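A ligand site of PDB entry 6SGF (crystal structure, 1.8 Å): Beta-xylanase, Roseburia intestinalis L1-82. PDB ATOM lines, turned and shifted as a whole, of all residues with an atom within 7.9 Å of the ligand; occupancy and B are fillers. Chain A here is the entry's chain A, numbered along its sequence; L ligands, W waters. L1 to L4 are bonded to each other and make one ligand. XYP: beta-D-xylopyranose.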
ATOM      1  N   TRP A  18     -11.903  21.504  14.897  1.00  0.00           N
ATOM      2  CA  TRP A  18     -12.413  20.789  13.743  1.00  0.00           C
ATOM      3  C   TRP A  18     -11.637  21.294  12.532  1.00  0.00           C
ATOM      4  O   TRP A  18     -11.330  22.487  12.442  1.00  0.00           O
ATOM      5  CB  TRP A  18     -13.923  21.042  13.567  1.00  0.00           C
ATOM      6  CG  TRP A  18     -14.623  20.152  12.613  1.00  0.00           C
ATOM      7  CD1 TRP A  18     -15.314  18.998  12.924  1.00  0.00           C
ATOM      8  CD2 TRP A  18     -14.791  20.339  11.200  1.00  0.00           C
ATOM      9  NE1 TRP A  18     -15.881  18.464  11.791  1.00  0.00           N
ATOM     10  CE2 TRP A  18     -15.564  19.256  10.722  1.00  0.00           C
ATOM     11  CE3 TRP A  18     -14.345  21.300  10.302  1.00  0.00           C
ATOM     12  CZ2 TRP A  18     -15.904  19.116   9.380  1.00  0.00           C
ATOM     13  CZ3 TRP A  18     -14.692  21.167   8.970  1.00  0.00           C
ATOM     14  CH2 TRP A  18     -15.447  20.076   8.530  1.00  0.00           C
ATOM     15  N   ASP A  20     -11.157  19.997   8.136  1.00  0.00           N
ATOM     16  CA  ASP A  20     -10.944  19.050   7.047  1.00  0.00           C
ATOM     17  C   ASP A  20      -9.865  19.511   6.101  1.00  0.00           C
ATOM     18  O   ASP A  20      -9.529  18.776   5.168  1.00  0.00           O
ATOM     19  CB  ASP A  20     -12.260  18.757   6.304  1.00  0.00           C
ATOM     20  CG  ASP A  20     -12.946  19.982   5.760  1.00  0.00           C
ATOM     21  OD1 ASP A  20     -12.439  21.120   5.891  1.00  0.00           O
ATOM     22  OD2 ASP A  20     -14.052  19.782   5.190  1.00  0.00           O
ATOM     23  N   GLN A  37     -12.690  22.501  -2.266  1.00  0.00           N
ATOM     24  CA  GLN A  37     -13.551  23.657  -2.014  1.00  0.00           C
ATOM     25  C   GLN A  37     -14.225  23.518  -0.660  1.00  0.00           C
ATOM     26  O   GLN A  37     -14.697  22.450  -0.284  1.00  0.00           O
ATOM     27  CB  GLN A  37     -14.640  23.782  -3.103  1.00  0.00           C
ATOM     28  CG  GLN A  37     -15.479  25.087  -2.971  1.00  0.00           C
ATOM     29  CD  GLN A  37     -16.506  25.266  -4.055  1.00  0.00           C
ATOM     30  OE1 GLN A  37     -17.131  24.298  -4.489  1.00  0.00           O
ATOM     31  NE2 GLN A  37     -16.692  26.517  -4.504  1.00  0.00           N
ATOM     32  N   TYR A  38     -14.214  24.613   0.103  1.00  0.00           N
ATOM     33  CA  TYR A  38     -14.839  24.763   1.426  1.00  0.00           C
ATOM     34  C   TYR A  38     -14.087  24.029   2.539  1.00  0.00           C
ATOM     35  O   TYR A  38     -14.518  24.095   3.709  1.00  0.00           O
ATOM     36  CB  TYR A  38     -16.314  24.337   1.416  1.00  0.00           C
ATOM     37  CG  TYR A  38     -17.143  25.206   0.494  1.00  0.00           C
ATOM     38  CD1 TYR A  38     -16.991  26.579   0.486  1.00  0.00           C
ATOM     39  CD2 TYR A  38     -18.076  24.662  -0.401  1.00  0.00           C
ATOM     40  CE1 TYR A  38     -17.745  27.393  -0.365  1.00  0.00           C
ATOM     41  CE2 TYR A  38     -18.854  25.489  -1.258  1.00  0.00           C
ATOM     42  CZ  TYR A  38     -18.683  26.844  -1.218  1.00  0.00           C
ATOM     43  OH  TYR A  38     -19.431  27.697  -2.013  1.00  0.00           O
ATOM     44  N   ASN A  39     -12.940  23.411   2.247  1.00  0.00           N
ATOM     45  CA  ASN A  39     -12.057  22.883   3.287  1.00  0.00           C
ATOM     46  C   ASN A  39     -11.718  24.013   4.256  1.00  0.00           C
ATOM     47  O   ASN A  39     -11.586  25.173   3.855  1.00  0.00           O
ATOM     48  CB  ASN A  39     -10.762  22.361   2.692  1.00  0.00           C
ATOM     49  CG  ASN A  39     -10.779  20.890   2.243  1.00  0.00           C
ATOM     50  OD1 ASN A  39      -9.758  20.448   1.757  1.00  0.00           O
ATOM     51  ND2 ASN A  39     -11.878  20.161   2.374  1.00  0.00           N
ATOM     52  N   GLN A  40     -11.610  23.678   5.531  1.00  0.00           N
ATOM     53  CA  GLN A  40     -11.487  24.738   6.517  1.00  0.00           C
ATOM     54  C   GLN A  40     -10.940  24.177   7.823  1.00  0.00           C
ATOM     55  O   GLN A  40     -10.934  22.966   8.066  1.00  0.00           O
ATOM     56  CB  GLN A  40     -12.831  25.436   6.783  1.00  0.00           C
ATOM     57  CG  GLN A  40     -13.859  24.506   7.357  1.00  0.00           C
ATOM     58  CD  GLN A  40     -15.224  25.157   7.481  1.00  0.00           C
ATOM     59  OE1 GLN A  40     -15.387  26.215   8.077  1.00  0.00           O
ATOM     60  NE2 GLN A  40     -16.210  24.531   6.899  1.00  0.00           N
ATOM     61  N   SER A  69     -11.335  32.885   3.250  1.00  0.00           N
ATOM     62  CA  SER A  69     -12.521  33.318   3.967  1.00  0.00           C
ATOM     63  C   SER A  69     -12.265  33.197   5.464  1.00  0.00           C
ATOM     64  O   SER A  69     -11.621  32.255   5.908  1.00  0.00           O
ATOM     65  CB  SER A  69     -13.714  32.446   3.572  1.00  0.00           C
ATOM     66  OG  SER A  69     -13.961  32.655   2.188  1.00  0.00           O
ATOM     67  N   LYS A  71     -13.833  33.567   9.549  1.00  0.00           N
ATOM     68  CA  LYS A  71     -15.029  33.314  10.334  1.00  0.00           C
ATOM     69  C   LYS A  71     -14.797  33.638  11.801  1.00  0.00           C
ATOM     70  O   LYS A  71     -13.747  33.284  12.353  1.00  0.00           O
ATOM     71  CB  LYS A  71     -15.460  31.836  10.249  1.00  0.00           C
ATOM     72  CG  LYS A  71     -15.959  31.364   8.860  1.00  0.00           C
ATOM     73  CD  LYS A  71     -16.492  29.917   8.940  1.00  0.00           C
ATOM     74  CE  LYS A  71     -16.865  29.451   7.526  1.00  0.00           C
ATOM     75  NZ  LYS A  71     -17.464  28.073   7.531  1.00  0.00           N
ATOM     76  N   TYR A  73     -16.945  32.701  15.152  1.00  0.00           N
ATOM     77  CA  TYR A  73     -18.042  31.873  15.635  1.00  0.00           C
ATOM     78  C   TYR A  73     -18.658  32.516  16.875  1.00  0.00           C
ATOM     79  O   TYR A  73     -17.990  33.256  17.613  1.00  0.00           O
ATOM     80  CB  TYR A  73     -17.582  30.455  15.987  1.00  0.00           C
ATOM     81  CG  TYR A  73     -17.205  29.610  14.801  1.00  0.00           C
ATOM     82  CD1 TYR A  73     -15.975  29.786  14.165  1.00  0.00           C
ATOM     83  CD2 TYR A  73     -18.046  28.631  14.321  1.00  0.00           C
ATOM     84  CE1 TYR A  73     -15.610  29.006  13.034  1.00  0.00           C
ATOM     85  CE2 TYR A  73     -17.699  27.852  13.228  1.00  0.00           C
ATOM     86  CZ  TYR A  73     -16.490  28.054  12.568  1.00  0.00           C
ATOM     87  OH  TYR A  73     -16.176  27.274  11.472  1.00  0.00           O
ATOM     88  N   ASP A  77     -23.435  26.068  14.925  1.00  0.00           N
ATOM     89  CA  ASP A  77     -22.700  25.016  14.239  1.00  0.00           C
ATOM     90  C   ASP A  77     -21.827  25.590  13.117  1.00  0.00           C
ATOM     91  O   ASP A  77     -20.830  24.969  12.731  1.00  0.00           O
ATOM     92  CB  ASP A  77     -23.659  23.930  13.741  1.00  0.00           C
ATOM     93  CG  ASP A  77     -24.000  22.935  14.828  1.00  0.00           C
ATOM     94  OD1 ASP A  77     -23.862  23.295  16.011  1.00  0.00           O
ATOM     95  OD2 ASP A  77     -24.414  21.798  14.502  1.00  0.00           O
ATOM     96  N   ASP A  78     -22.203  26.739  12.555  1.00  0.00           N
ATOM     97  CA  ASP A  78     -21.310  27.459  11.654  1.00  0.00           C
ATOM     98  C   ASP A  78     -21.315  28.924  12.082  1.00  0.00           C
ATOM     99  O   ASP A  78     -22.222  29.387  12.774  1.00  0.00           O
ATOM    100  CB  ASP A  78     -21.748  27.317  10.184  1.00  0.00           C
ATOM    101  CG  ASP A  78     -20.587  27.461   9.181  1.00  0.00           C
ATOM    102  OD1 ASP A  78     -19.489  27.958   9.544  1.00  0.00           O
ATOM    103  OD2 ASP A  78     -20.775  27.060   8.012  1.00  0.00           O
ATOM    104  N   ALA A  79     -20.354  29.670  11.601  1.00  0.00           N
ATOM    105  CA  ALA A  79     -20.381  31.106  11.803  1.00  0.00           C
ATOM    106  C   ALA A  79     -21.484  31.705  10.958  1.00  0.00           C
ATOM    107  O   ALA A  79     -21.820  31.208   9.872  1.00  0.00           O
ATOM    108  CB  ALA A  79     -19.032  31.729  11.414  1.00  0.00           C
ATOM    109  N   ALA A  81     -23.274  34.476   8.455  1.00  0.00           N
ATOM    110  CA  ALA A  81     -22.778  35.225   7.303  1.00  0.00           C
ATOM    111  C   ALA A  81     -22.285  36.607   7.710  1.00  0.00           C
ATOM    112  O   ALA A  81     -21.283  37.096   7.171  1.00  0.00           O
ATOM    113  CB  ALA A  81     -23.873  35.346   6.232  1.00  0.00           C
ATOM    114  N   THR A  84     -18.635  36.499   8.766  1.00  0.00           N
ATOM    115  CA  THR A  84     -17.764  35.813   7.817  1.00  0.00           C
ATOM    116  C   THR A  84     -17.419  36.820   6.735  1.00  0.00           C
ATOM    117  O   THR A  84     -18.244  37.672   6.418  1.00  0.00           O
ATOM    118  CB  THR A  84     -18.464  34.580   7.187  1.00  0.00           C
ATOM    119  OG1 THR A  84     -18.867  33.673   8.227  1.00  0.00           O
ATOM    120  CG2 THR A  84     -17.555  33.839   6.173  1.00  0.00           C
ATOM    121  N   GLN A  85     -16.202  36.775   6.226  1.00  0.00           N
ATOM    122  CA  GLN A  85     -15.825  37.535   5.052  1.00  0.00           C
ATOM    123  C   GLN A  85     -15.218  36.565   4.048  1.00  0.00           C
ATOM    124  O   GLN A  85     -14.458  35.680   4.453  1.00  0.00           O
ATOM    125  CB  GLN A  85     -14.843  38.622   5.405  1.00  0.00           C
ATOM    126  CG  GLN A  85     -15.365  39.610   6.436  1.00  0.00           C
ATOM    127  CD  GLN A  85     -15.888  40.863   5.797  1.00  0.00           C
ATOM    128  OE1 GLN A  85     -15.113  41.761   5.457  1.00  0.00           O
ATOM    129  NE2 GLN A  85     -17.205  40.931   5.608  1.00  0.00           N
ATOM    130  N   TYR A  86     -15.546  36.722   2.773  1.00  0.00           N
ATOM    131  CA  TYR A  86     -15.128  35.770   1.743  1.00  0.00           C
ATOM    132  C   TYR A  86     -14.150  36.382   0.738  1.00  0.00           C
ATOM    133  O   TYR A  86     -14.180  37.576   0.459  1.00  0.00           O
ATOM    134  CB  TYR A  86     -16.332  35.245   0.944  1.00  0.00           C
ATOM    135  CG  TYR A  86     -17.425  34.608   1.774  1.00  0.00           C
ATOM    136  CD1 TYR A  86     -17.316  33.290   2.187  1.00  0.00           C
ATOM    137  CD2 TYR A  86     -18.565  35.301   2.099  1.00  0.00           C
ATOM    138  CE1 TYR A  86     -18.330  32.689   2.948  1.00  0.00           C
ATOM    139  CE2 TYR A  86     -19.574  34.724   2.856  1.00  0.00           C
ATOM    140  CZ  TYR A  86     -19.444  33.402   3.276  1.00  0.00           C
ATOM    141  OH  TYR A  86     -20.439  32.799   4.022  1.00  0.00           O
ATOM    142  N   GLY A  87     -13.303  35.529   0.191  1.00  0.00           N
ATOM    143  CA  GLY A  87     -12.471  35.854  -0.943  1.00  0.00           C
ATOM    144  C   GLY A  87     -11.421  36.914  -0.713  1.00  0.00           C
ATOM    145  O   GLY A  87     -11.120  37.674  -1.631  1.00  0.00           O
ATOM    146  N   MET A 110     -11.275  29.394   5.823  1.00  0.00           N
ATOM    147  CA  MET A 110     -11.876  28.503   4.809  1.00  0.00           C
ATOM    148  C   MET A 110     -11.434  28.965   3.432  1.00  0.00           C
ATOM    149  O   MET A 110     -11.119  30.151   3.233  1.00  0.00           O
ATOM    150  CB  MET A 110     -13.423  28.506   4.855  1.00  0.00           C
ATOM    151  CG  MET A 110     -14.153  27.676   3.826  1.00  0.00           C
ATOM    152  SD  MET A 110     -15.919  27.771   4.172  1.00  0.00           S
ATOM    153  CE  MET A 110     -16.239  29.463   3.635  1.00  0.00           C
ATOM    154  N   ILE A 111     -11.417  28.043   2.447  1.00  0.00           N
ATOM    155  CA  ILE A 111     -11.253  28.457   1.057  1.00  0.00           C
ATOM    156  C   ILE A 111     -12.565  28.242   0.303  1.00  0.00           C
ATOM    157  O   ILE A 111     -13.312  27.297   0.566  1.00  0.00           O
ATOM    158  CB  ILE A 111     -10.089  27.750   0.330  1.00  0.00           C
ATOM    159  CG1 ILE A 111     -10.259  26.232   0.328  1.00  0.00           C
ATOM    160  CG2 ILE A 111      -8.728  28.192   0.928  1.00  0.00           C
ATOM    161  CD1 ILE A 111      -9.671  25.599  -0.909  1.00  0.00           C
ATOM    162  N   THR A 112     -12.826  29.120  -0.656  1.00  0.00           N
ATOM    163  CA  THR A 112     -13.975  28.977  -1.537  1.00  0.00           C
ATOM    164  C   THR A 112     -13.562  28.607  -2.945  1.00  0.00           C
ATOM    165  O   THR A 112     -14.425  28.430  -3.820  1.00  0.00           O
ATOM    166  CB  THR A 112     -14.780  30.290  -1.577  1.00  0.00           C
ATOM    167  OG1 THR A 112     -13.921  31.349  -2.032  1.00  0.00           O
ATOM    168  CG2 THR A 112     -15.332  30.633  -0.199  1.00  0.00           C
ATOM    169  N   GLU A 113     -12.283  28.518  -3.218  1.00  0.00           N
ATOM    170  CA  GLU A 113     -11.763  28.149  -4.561  1.00  0.00           C
ATOM    171  C   GLU A 113     -12.325  26.796  -4.988  1.00  0.00           C
ATOM    172  O   GLU A 113     -12.227  25.859  -4.253  1.00  0.00           O
ATOM    173  CB  GLU A 113     -10.238  28.133  -4.552  1.00  0.00           C
ATOM    174  CG  GLU A 113      -9.616  27.476  -5.748  1.00  0.00           C
ATOM    175  CD  GLU A 113     -10.081  27.966  -7.106  1.00  0.00           C
ATOM    176  OE1 GLU A 113     -10.310  29.158  -7.233  1.00  0.00           O
ATOM    177  OE2 GLU A 113     -10.200  27.135  -8.011  1.00  0.00           O
HETATM  178  C1  XYP L   1     -19.930  27.161   3.291  1.00  0.00           C
HETATM  179  C2  XYP L   1     -19.690  27.045   4.795  1.00  0.00           C
HETATM  180  C3  XYP L   1     -18.867  25.868   5.141  1.00  0.00           C
HETATM  181  C4  XYP L   1     -19.538  24.700   4.506  1.00  0.00           C
HETATM  182  C5  XYP L   1     -19.712  24.778   2.986  1.00  0.00           C
HETATM  183  O2  XYP L   1     -19.017  28.238   5.194  1.00  0.00           O
HETATM  184  O3  XYP L   1     -18.842  25.658   6.579  1.00  0.00           O
HETATM  185  O4  XYP L   1     -18.810  23.516   4.790  1.00  0.00           O
HETATM  186  O5  XYP L   1     -20.543  25.938   2.665  1.00  0.00           O
HETATM  187  C1  XYP L   2     -20.614  31.422   0.251  1.00  0.00           C
HETATM  188  C2  XYP L   2     -21.950  30.690   0.397  1.00  0.00           C
HETATM  189  C3  XYP L   2     -21.992  29.884   1.651  1.00  0.00           C
HETATM  190  C4  XYP L   2     -20.833  28.963   1.753  1.00  0.00           C
HETATM  191  C5  XYP L   2     -19.526  29.753   1.675  1.00  0.00           C
HETATM  192  O2  XYP L   2     -23.001  31.662   0.495  1.00  0.00           O
HETATM  193  O3  XYP L   2     -23.203  29.067   1.715  1.00  0.00           O
HETATM  194  O4  XYP L   2     -20.800  28.262   2.995  1.00  0.00           O
HETATM  195  O5  XYP L   2     -19.441  30.468   0.417  1.00  0.00           O
HETATM  196  C1  XYP L   3     -19.654  35.810  -2.377  1.00  0.00           C
HETATM  197  C2  XYP L   3     -18.558  34.745  -2.457  1.00  0.00           C
HETATM  198  C3  XYP L   3     -19.105  33.370  -2.298  1.00  0.00           C
HETATM  199  C4  XYP L   3     -19.946  33.258  -1.071  1.00  0.00           C
HETATM  200  C5  XYP L   3     -21.033  34.326  -0.986  1.00  0.00           C
HETATM  201  O2  XYP L   3     -17.906  34.939  -3.707  1.00  0.00           O
HETATM  202  O3  XYP L   3     -17.998  32.489  -2.141  1.00  0.00           O
HETATM  203  O4  XYP L   3     -20.522  31.950  -1.040  1.00  0.00           O
HETATM  204  O5  XYP L   3     -20.505  35.684  -1.168  1.00  0.00           O
HETATM  205  O1  XYP L   4     -21.058  41.329  -5.768  1.00  0.00           O
HETATM  206  C1  XYP L   4     -20.282  40.482  -5.038  1.00  0.00           C
HETATM  207  C2  XYP L   4     -20.456  40.759  -3.536  1.00  0.00           C
HETATM  208  C3  XYP L   4     -19.695  39.758  -2.718  1.00  0.00           C
HETATM  209  C4  XYP L   4     -20.136  38.350  -3.000  1.00  0.00           C
HETATM  210  C5  XYP L   4     -20.009  38.033  -4.498  1.00  0.00           C
HETATM  211  O2  XYP L   4     -20.011  42.092  -3.237  1.00  0.00           O
HETATM  212  O3  XYP L   4     -19.863  40.035  -1.301  1.00  0.00           O
HETATM  213  O4  XYP L   4     -19.334  37.424  -2.246  1.00  0.00           O
HETATM  214  O5  XYP L   4     -20.625  39.052  -5.387  1.00  0.00           O
HETATM  215  O   HOH W   1     -18.470  30.106  -3.175  1.00  0.00           O
HETATM  216  O   HOH W   2     -20.386  30.507   5.398  1.00  0.00           O
HETATM  217  O   HOH W   3     -22.936  33.424   2.914  1.00  0.00           O
HETATM  218  O   HOH W   4     -15.589  33.340  -2.824  1.00  0.00           O
HETATM  219  O   HOH W   5     -17.428  39.262  -0.542  1.00  0.00           O
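The side-chain amide nitrogen (NE2) of Gln 40 is in hydrogen-bond range of an oxygen (O3) of XYP L1, 2.9 Å away.
The side-chain amino group (NZ) of Lys 71 lies within hydrogen-bond range of an oxygen (O2) of XYP L1 (2.8 Å).
An oxygen (O2) of XYP L1 sits at hydrogen-bond distance from the side-chain sulfur of Met 110.
The side-chain carboxylate (OD2) of Asp 78 is in hydrogen-bond range of an oxygen (O3) of XYP L1 (2.8 Å).
Residues that only touch the ligand: Tyr 38 (3.6 Å), Tyr 86 (3.4 Å) and Thr 112 (3.8 Å).
Seven residues have an atom within 4 Å of the ligand: Tyr 38, Gln 40, Lys 71, Asp 78, Tyr 86, Met 110 and Thr 112.
Water W1 bridges an oxygen (O3) of XYP L3 (2.6 Å) and the side-chain hydroxyl of Tyr 38 (2.8 Å).
Water W4 lies within hydrogen-bond range of O3 of XYP L3 (2.6 Å) and OG1 of Thr 112 (2.7 Å).
Water W2 lies within hydrogen-bond range of an oxygen (O2) of XYP L1 (2.7 Å) and the side-chain hydroxyl (OH) of Tyr 86 (2.7 Å).
Water W3 lies within hydrogen-bond range of the side-chain hydroxyl (OH) of Tyr 86 (2.8 Å) and an oxygen (O2) of XYP L2 (3.0 Å).
The side-chain amino group of Lys 71 is in hydrogen-bond range of the side-chain amide oxygen of Gln 40 (2.8 Å).
The backbone carbonyl oxygen (O) of Ile 111 lies within hydrogen-bond range of the backbone NH (N) of Tyr 38.
The side-chain carboxylate (OD1) of Asp 78 lies within salt-bridge range of the side-chain amino group (NZ) of Lys 71 (2.9 Å).
The side-chain carboxylate of Asp 20 is in hydrogen-bond range of the backbone NH of Gln 40, at 2.7 Å.
The side-chain amino group (NZ) of Lys 71 is in hydrogen-bond range of the side-chain sulfur (SD) of Met 110 (3.7 Å).
The backbone NH (N) of Ser 69 lies within hydrogen-bond range of the backbone carbonyl oxygen (O) of Met 110, at 2.7 Å.
The side-chain amide nitrogen of Gln 37 lies within hydrogen-bond range of the backbone carbonyl oxygen of Thr 112 (3.0 Å).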
